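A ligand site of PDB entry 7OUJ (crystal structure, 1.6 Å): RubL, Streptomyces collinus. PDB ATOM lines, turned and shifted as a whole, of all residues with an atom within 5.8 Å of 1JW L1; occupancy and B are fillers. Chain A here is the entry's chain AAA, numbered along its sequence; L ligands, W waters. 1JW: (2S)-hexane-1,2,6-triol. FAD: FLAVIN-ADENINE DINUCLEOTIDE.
An oxygen (O1A) of FAD L2 is in salt-bridge range of the guanidinium group (NH2) of Arg 53 (2.9 Å).
An oxygen (O4) of FAD L2 lies within hydrogen-bond range of the backbone NH (N) of Val 55.
O09 of 1JW L1 is in hydrogen-bond range of OG1 of Thr 245.
O of Pro 52 lies within hydrogen-bond range of O09 of 1JW L1 (2.6 Å).
The backbone carbonyl oxygen (O) of Arg 53 is in hydrogen-bond range of an oxygen (O08) of 1JW L1 (2.6 Å).
O of Val 236 is in hydrogen-bond range of N of Thr 245.
N of Asp 238 sits at hydrogen-bond distance from O of Gly 243 (2.9 Å).
The guanidinium group (NH1) of Arg 53 lies within hydrogen-bond range of the backbone carbonyl oxygen (O) of His 51 (2.9 Å).
Residues that only touch 1JW L1: Val 236 (3.2 Å), Gly 244 (3.5 Å), Asp 238 (3.8 Å) and Pro 122 (3.9 Å).
Hydrophobic or aromatic side chains that line 1JW L1: Pro 52, Pro 122 and Val 236.
Water W1 lies within hydrogen-bond range of an oxygen (O04) of 1JW L1, the side-chain hydroxyl of Thr 245 and the backbone carbonyl oxygen of Gly 244.
Water W3 lies within hydrogen-bond range of an oxygen (O08) of 1JW L1, the side-chain hydroxyl (OG) of Ser 205 and the backbone carbonyl oxygen (O) of Pro 52.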
ATOM      1  N   HIS A  51      10.456 -25.451  -1.853  1.00  0.00           N
ATOM      2  CA  HIS A  51       9.287 -25.597  -0.962  1.00  0.00           C
ATOM      3  C   HIS A  51       8.767 -24.205  -0.635  1.00  0.00           C
ATOM      4  O   HIS A  51       9.462 -23.445   0.055  1.00  0.00           O
ATOM      5  CB  HIS A  51       9.636 -26.411   0.275  1.00  0.00           C
ATOM      6  CG  HIS A  51       8.439 -26.678   1.114  1.00  0.00           C
ATOM      7  ND1 HIS A  51       7.892 -25.734   1.967  1.00  0.00           N
ATOM      8  CD2 HIS A  51       7.636 -27.760   1.168  1.00  0.00           C
ATOM      9  CE1 HIS A  51       6.815 -26.237   2.523  1.00  0.00           C
ATOM     10  NE2 HIS A  51       6.646 -27.470   2.057  1.00  0.00           N
ATOM     11  N   PRO A  52       7.520 -23.875  -0.990  1.00  0.00           N
ATOM     12  CA  PRO A  52       7.031 -22.531  -0.706  1.00  0.00           C
ATOM     13  C   PRO A  52       6.598 -22.529   0.750  1.00  0.00           C
ATOM     14  O   PRO A  52       5.905 -23.434   1.155  1.00  0.00           O
ATOM     15  CB  PRO A  52       5.862 -22.378  -1.656  1.00  0.00           C
ATOM     16  CG  PRO A  52       5.346 -23.759  -1.836  1.00  0.00           C
ATOM     17  CD  PRO A  52       6.555 -24.690  -1.733  1.00  0.00           C
ATOM     18  N   ARG A  53       6.933 -21.459   1.480  1.00  0.00           N
ATOM     19  CA  ARG A  53       6.399 -21.257   2.834  1.00  0.00           C
ATOM     20  C   ARG A  53       5.349 -20.162   2.756  1.00  0.00           C
ATOM     21  O   ARG A  53       4.183 -20.438   3.039  1.00  0.00           O
ATOM     22  CB  ARG A  53       7.490 -20.848   3.814  1.00  0.00           C
ATOM     23  CG  ARG A  53       8.386 -21.994   4.248  1.00  0.00           C
ATOM     24  CD  ARG A  53       9.484 -22.307   3.245  1.00  0.00           C
ATOM     25  NE  ARG A  53      10.567 -21.318   3.313  1.00  0.00           N
ATOM     26  CZ  ARG A  53      11.452 -21.039   2.350  1.00  0.00           C
ATOM     27  NH1 ARG A  53      11.453 -21.673   1.204  1.00  0.00           N
ATOM     28  NH2 ARG A  53      12.378 -20.112   2.556  1.00  0.00           N
ATOM     29  N   ALA A  54       5.774 -18.956   2.383  1.00  0.00           N
ATOM     30  CA  ALA A  54       4.846 -17.809   2.359  1.00  0.00           C
ATOM     31  C   ALA A  54       3.834 -17.965   1.229  1.00  0.00           C
ATOM     32  O   ALA A  54       4.149 -18.458   0.158  1.00  0.00           O
ATOM     33  CB  ALA A  54       5.601 -16.510   2.247  1.00  0.00           C
ATOM     34  N   VAL A  55       2.642 -17.451   1.450  1.00  0.00           N
ATOM     35  CA  VAL A  55       1.592 -17.426   0.417  1.00  0.00           C
ATOM     36  C   VAL A  55       0.869 -16.088   0.462  1.00  0.00           C
ATOM     37  O   VAL A  55       0.368 -15.705  -0.569  1.00  0.00           O
ATOM     38  CB  VAL A  55       0.628 -18.629   0.570  1.00  0.00           C
ATOM     39  CG1 VAL A  55      -0.179 -18.529   1.838  1.00  0.00           C
ATOM     40  CG2 VAL A  55      -0.273 -18.760  -0.640  1.00  0.00           C
ATOM     41  N   PHE A  81      -5.204 -18.043  -7.898  1.00  0.00           N
ATOM     42  CA  PHE A  81      -5.414 -17.940  -6.439  1.00  0.00           C
ATOM     43  C   PHE A  81      -6.416 -16.864  -6.090  1.00  0.00           C
ATOM     44  O   PHE A  81      -6.904 -16.861  -4.943  1.00  0.00           O
ATOM     45  CB  PHE A  81      -4.076 -17.680  -5.742  1.00  0.00           C
ATOM     46  CG  PHE A  81      -3.230 -18.914  -5.663  1.00  0.00           C
ATOM     47  CD1 PHE A  81      -3.430 -19.796  -4.611  1.00  0.00           C
ATOM     48  CD2 PHE A  81      -2.234 -19.160  -6.578  1.00  0.00           C
ATOM     49  CE1 PHE A  81      -2.642 -20.917  -4.486  1.00  0.00           C
ATOM     50  CE2 PHE A  81      -1.476 -20.298  -6.474  1.00  0.00           C
ATOM     51  CZ  PHE A  81      -1.677 -21.168  -5.430  1.00  0.00           C
ATOM     52  N   PRO A 122       2.184 -18.396  -3.932  1.00  0.00           N
ATOM     53  CA  PRO A 122       3.184 -19.166  -3.228  1.00  0.00           C
ATOM     54  C   PRO A 122       4.560 -18.527  -3.437  1.00  0.00           C
ATOM     55  O   PRO A 122       4.909 -18.085  -4.527  1.00  0.00           O
ATOM     56  CB  PRO A 122       3.089 -20.541  -3.910  1.00  0.00           C
ATOM     57  CG  PRO A 122       1.672 -20.604  -4.370  1.00  0.00           C
ATOM     58  CD  PRO A 122       1.382 -19.213  -4.848  1.00  0.00           C
ATOM     59  N   SER A 205       5.903 -29.134   7.080  1.00  0.00           N
ATOM     60  CA  SER A 205       5.083 -28.790   5.899  1.00  0.00           C
ATOM     61  C   SER A 205       5.275 -29.863   4.829  1.00  0.00           C
ATOM     62  O   SER A 205       6.441 -30.163   4.487  1.00  0.00           O
ATOM     63  CB  SER A 205       5.440 -27.444   5.390  1.00  0.00           C
ATOM     64  OG  SER A 205       4.952 -26.468   6.306  1.00  0.00           O
ATOM     65  N   VAL A 236      -3.389 -26.072   2.384  1.00  0.00           N
ATOM     66  CA  VAL A 236      -3.460 -24.981   1.405  1.00  0.00           C
ATOM     67  C   VAL A 236      -3.390 -25.627   0.039  1.00  0.00           C
ATOM     68  O   VAL A 236      -2.358 -26.251  -0.267  1.00  0.00           O
ATOM     69  CB  VAL A 236      -2.338 -23.957   1.601  1.00  0.00           C
ATOM     70  CG1 VAL A 236      -2.541 -22.799   0.638  1.00  0.00           C
ATOM     71  CG2 VAL A 236      -2.322 -23.443   3.033  1.00  0.00           C
ATOM     72  N   HIS A 237      -4.485 -25.570  -0.707  1.00  0.00           N
ATOM     73  CA  HIS A 237      -4.506 -26.195  -2.059  1.00  0.00           C
ATOM     74  C   HIS A 237      -3.984 -25.194  -3.090  1.00  0.00           C
ATOM     75  O   HIS A 237      -4.148 -23.983  -2.904  1.00  0.00           O
ATOM     76  CB  HIS A 237      -5.886 -26.780  -2.408  1.00  0.00           C
ATOM     77  CG  HIS A 237      -6.997 -25.824  -2.668  1.00  0.00           C
ATOM     78  ND1 HIS A 237      -7.093 -25.078  -3.842  1.00  0.00           N
ATOM     79  CD2 HIS A 237      -8.103 -25.567  -1.952  1.00  0.00           C
ATOM     80  CE1 HIS A 237      -8.206 -24.356  -3.791  1.00  0.00           C
ATOM     81  NE2 HIS A 237      -8.836 -24.643  -2.644  1.00  0.00           N
ATOM     82  N   ASP A 238      -3.367 -25.692  -4.144  1.00  0.00           N
ATOM     83  CA  ASP A 238      -2.846 -24.820  -5.219  1.00  0.00           C
ATOM     84  C   ASP A 238      -3.963 -24.344  -6.148  1.00  0.00           C
ATOM     85  O   ASP A 238      -5.167 -24.672  -5.941  1.00  0.00           O
ATOM     86  CB  ASP A 238      -1.673 -25.467  -5.955  1.00  0.00           C
ATOM     87  CG  ASP A 238      -1.986 -26.708  -6.748  1.00  0.00           C
ATOM     88  OD1 ASP A 238      -3.159 -26.903  -7.060  1.00  0.00           O
ATOM     89  OD2 ASP A 238      -1.066 -27.536  -6.898  1.00  0.00           O
ATOM     90  N   GLY A 243      -2.567 -30.210  -6.206  1.00  0.00           N
ATOM     91  CA  GLY A 243      -1.613 -30.391  -5.118  1.00  0.00           C
ATOM     92  C   GLY A 243      -1.805 -29.312  -4.093  1.00  0.00           C
ATOM     93  O   GLY A 243      -2.767 -28.566  -4.198  1.00  0.00           O
ATOM     94  N   GLY A 244      -0.891 -29.248  -3.153  1.00  0.00           N
ATOM     95  CA  GLY A 244      -0.980 -28.280  -2.046  1.00  0.00           C
ATOM     96  C   GLY A 244       0.056 -28.570  -1.003  1.00  0.00           C
ATOM     97  O   GLY A 244       0.970 -29.363  -1.270  1.00  0.00           O
ATOM     98  N   THR A 245      -0.158 -28.011   0.178  1.00  0.00           N
ATOM     99  CA  THR A 245       0.711 -28.245   1.334  1.00  0.00           C
ATOM    100  C   THR A 245      -0.171 -28.620   2.506  1.00  0.00           C
ATOM    101  O   THR A 245      -1.170 -27.951   2.728  1.00  0.00           O
ATOM    102  CB  THR A 245       1.584 -27.027   1.642  1.00  0.00           C
ATOM    103  OG1 THR A 245       2.365 -26.746   0.478  1.00  0.00           O
ATOM    104  CG2 THR A 245       2.454 -27.234   2.869  1.00  0.00           C
ATOM    105  N   ILE A 247       0.175 -28.941   6.526  1.00  0.00           N
ATOM    106  CA  ILE A 247       1.106 -28.545   7.627  1.00  0.00           C
ATOM    107  C   ILE A 247       0.605 -29.210   8.906  1.00  0.00           C
ATOM    108  O   ILE A 247      -0.565 -28.990   9.282  1.00  0.00           O
ATOM    109  CB  ILE A 247       1.153 -27.029   7.781  1.00  0.00           C
ATOM    110  CG1 ILE A 247       1.517 -26.354   6.456  1.00  0.00           C
ATOM    111  CG2 ILE A 247       2.098 -26.625   8.893  1.00  0.00           C
ATOM    112  CD1 ILE A 247       1.163 -24.857   6.442  1.00  0.00           C
HETATM  113  C01 1JW L   1       1.607 -23.239  -1.132  1.00  0.00           C
HETATM  114  C02 1JW L   1       0.335 -23.455  -2.016  1.00  0.00           C
HETATM  115  C03 1JW L   1      -0.071 -24.805  -2.050  1.00  0.00           C
HETATM  116  O04 1JW L   1       0.773 -25.432  -3.067  1.00  0.00           O
HETATM  117  C05 1JW L   1       1.307 -23.276   0.379  1.00  0.00           C
HETATM  118  C06 1JW L   1       2.566 -23.123   1.314  1.00  0.00           C
HETATM  119  C07 1JW L   1       2.114 -23.020   2.827  1.00  0.00           C
HETATM  120  O08 1JW L   1       3.261 -22.801   3.692  1.00  0.00           O
HETATM  121  O09 1JW L   1       3.410 -24.245   1.168  1.00  0.00           O
HETATM  122  PA  FAD L   2      14.455 -17.531   4.505  1.00  0.00           P
HETATM  123  O1A FAD L   2      13.186 -17.636   3.717  1.00  0.00           O
HETATM  124  O2A FAD L   2      14.638 -18.425   5.679  1.00  0.00           O
HETATM  125  O5B FAD L   2      15.659 -17.710   3.490  1.00  0.00           O
HETATM  126  C5B FAD L   2      17.015 -17.581   3.963  1.00  0.00           C
HETATM  127  C4B FAD L   2      17.899 -17.997   2.829  1.00  0.00           C
HETATM  128  O4B FAD L   2      19.279 -17.818   3.227  1.00  0.00           O
HETATM  129  C3B FAD L   2      17.727 -19.469   2.413  1.00  0.00           C
HETATM  130  O3B FAD L   2      17.440 -19.639   1.041  1.00  0.00           O
HETATM  131  C2B FAD L   2      19.069 -20.103   2.810  1.00  0.00           C
HETATM  132  O2B FAD L   2      19.475 -21.169   1.970  1.00  0.00           O
HETATM  133  C1B FAD L   2      20.016 -18.906   2.706  1.00  0.00           C
HETATM  134  N9A FAD L   2      21.242 -19.011   3.479  1.00  0.00           N
HETATM  135  C8A FAD L   2      21.307 -19.290   4.828  1.00  0.00           C
HETATM  136  N7A FAD L   2      22.550 -19.293   5.263  1.00  0.00           N
HETATM  137  C5A FAD L   2      23.325 -19.009   4.144  1.00  0.00           C
HETATM  138  C6A FAD L   2      24.704 -18.847   3.981  1.00  0.00           C
HETATM  139  N6A FAD L   2      25.587 -19.004   4.976  1.00  0.00           N
HETATM  140  N1A FAD L   2      25.159 -18.556   2.732  1.00  0.00           N
HETATM  141  C2A FAD L   2      24.261 -18.386   1.748  1.00  0.00           C
HETATM  142  N3A FAD L   2      22.943 -18.517   1.799  1.00  0.00           N
HETATM  143  C4A FAD L   2      22.524 -18.796   3.045  1.00  0.00           C
HETATM  144  N1  FAD L   2       5.162 -14.967   5.636  1.00  0.00           N
HETATM  145  C2  FAD L   2       4.314 -14.193   5.040  1.00  0.00           C
HETATM  146  O2  FAD L   2       4.524 -12.948   4.939  1.00  0.00           O
HETATM  147  N3  FAD L   2       3.134 -14.675   4.555  1.00  0.00           N
HETATM  148  C4  FAD L   2       2.741 -15.999   4.692  1.00  0.00           C
HETATM  149  O4  FAD L   2       1.670 -16.378   4.159  1.00  0.00           O
HETATM  150  C4X FAD L   2       3.611 -16.840   5.352  1.00  0.00           C
HETATM  151  N5  FAD L   2       3.283 -18.110   5.506  1.00  0.00           N
HETATM  152  C5X FAD L   2       4.209 -18.929   6.106  1.00  0.00           C
HETATM  153  C6  FAD L   2       3.900 -20.288   6.290  1.00  0.00           C
HETATM  154  C7  FAD L   2       4.799 -21.155   6.834  1.00  0.00           C
HETATM  155  C7M FAD L   2       4.435 -22.612   7.021  1.00  0.00           C
HETATM  156  C8  FAD L   2       6.050 -20.670   7.293  1.00  0.00           C
HETATM  157  C8M FAD L   2       7.067 -21.587   7.905  1.00  0.00           C
HETATM  158  C9  FAD L   2       6.358 -19.327   7.126  1.00  0.00           C
HETATM  159  C9A FAD L   2       5.461 -18.441   6.544  1.00  0.00           C
HETATM  160  N10 FAD L   2       5.744 -17.078   6.374  1.00  0.00           N
HETATM  161  C10 FAD L   2       4.844 -16.242   5.781  1.00  0.00           C
HETATM  162  C1' FAD L   2       7.067 -16.563   6.785  1.00  0.00           C
HETATM  163  C2' FAD L   2       8.053 -16.473   5.644  1.00  0.00           C
HETATM  164  O2' FAD L   2       8.234 -17.753   4.916  1.00  0.00           O
HETATM  165  C3' FAD L   2       9.424 -16.023   6.155  1.00  0.00           C
HETATM  166  O3' FAD L   2       9.245 -14.904   7.015  1.00  0.00           O
HETATM  167  C4' FAD L   2      10.368 -15.659   5.019  1.00  0.00           C
HETATM  168  O4' FAD L   2      10.632 -16.780   4.138  1.00  0.00           O
HETATM  169  C5' FAD L   2      11.691 -15.147   5.547  1.00  0.00           C
HETATM  170  O5' FAD L   2      12.457 -14.754   4.388  1.00  0.00           O
HETATM  171  P   FAD L   2      14.041 -14.601   4.538  1.00  0.00           P
HETATM  172  O1P FAD L   2      14.537 -14.329   3.170  1.00  0.00           O
HETATM  173  O2P FAD L   2      14.338 -13.691   5.667  1.00  0.00           O
HETATM  174  O3P FAD L   2      14.565 -16.026   5.096  1.00  0.00           O
HETATM  175  O   HOH W   1       2.766 -27.000  -2.257  1.00  0.00           O
HETATM  176  O   HOH W   2       1.529 -23.934  -5.973  1.00  0.00           O
HETATM  177  O   HOH W   3       5.193 -24.555   4.301  1.00  0.00           O
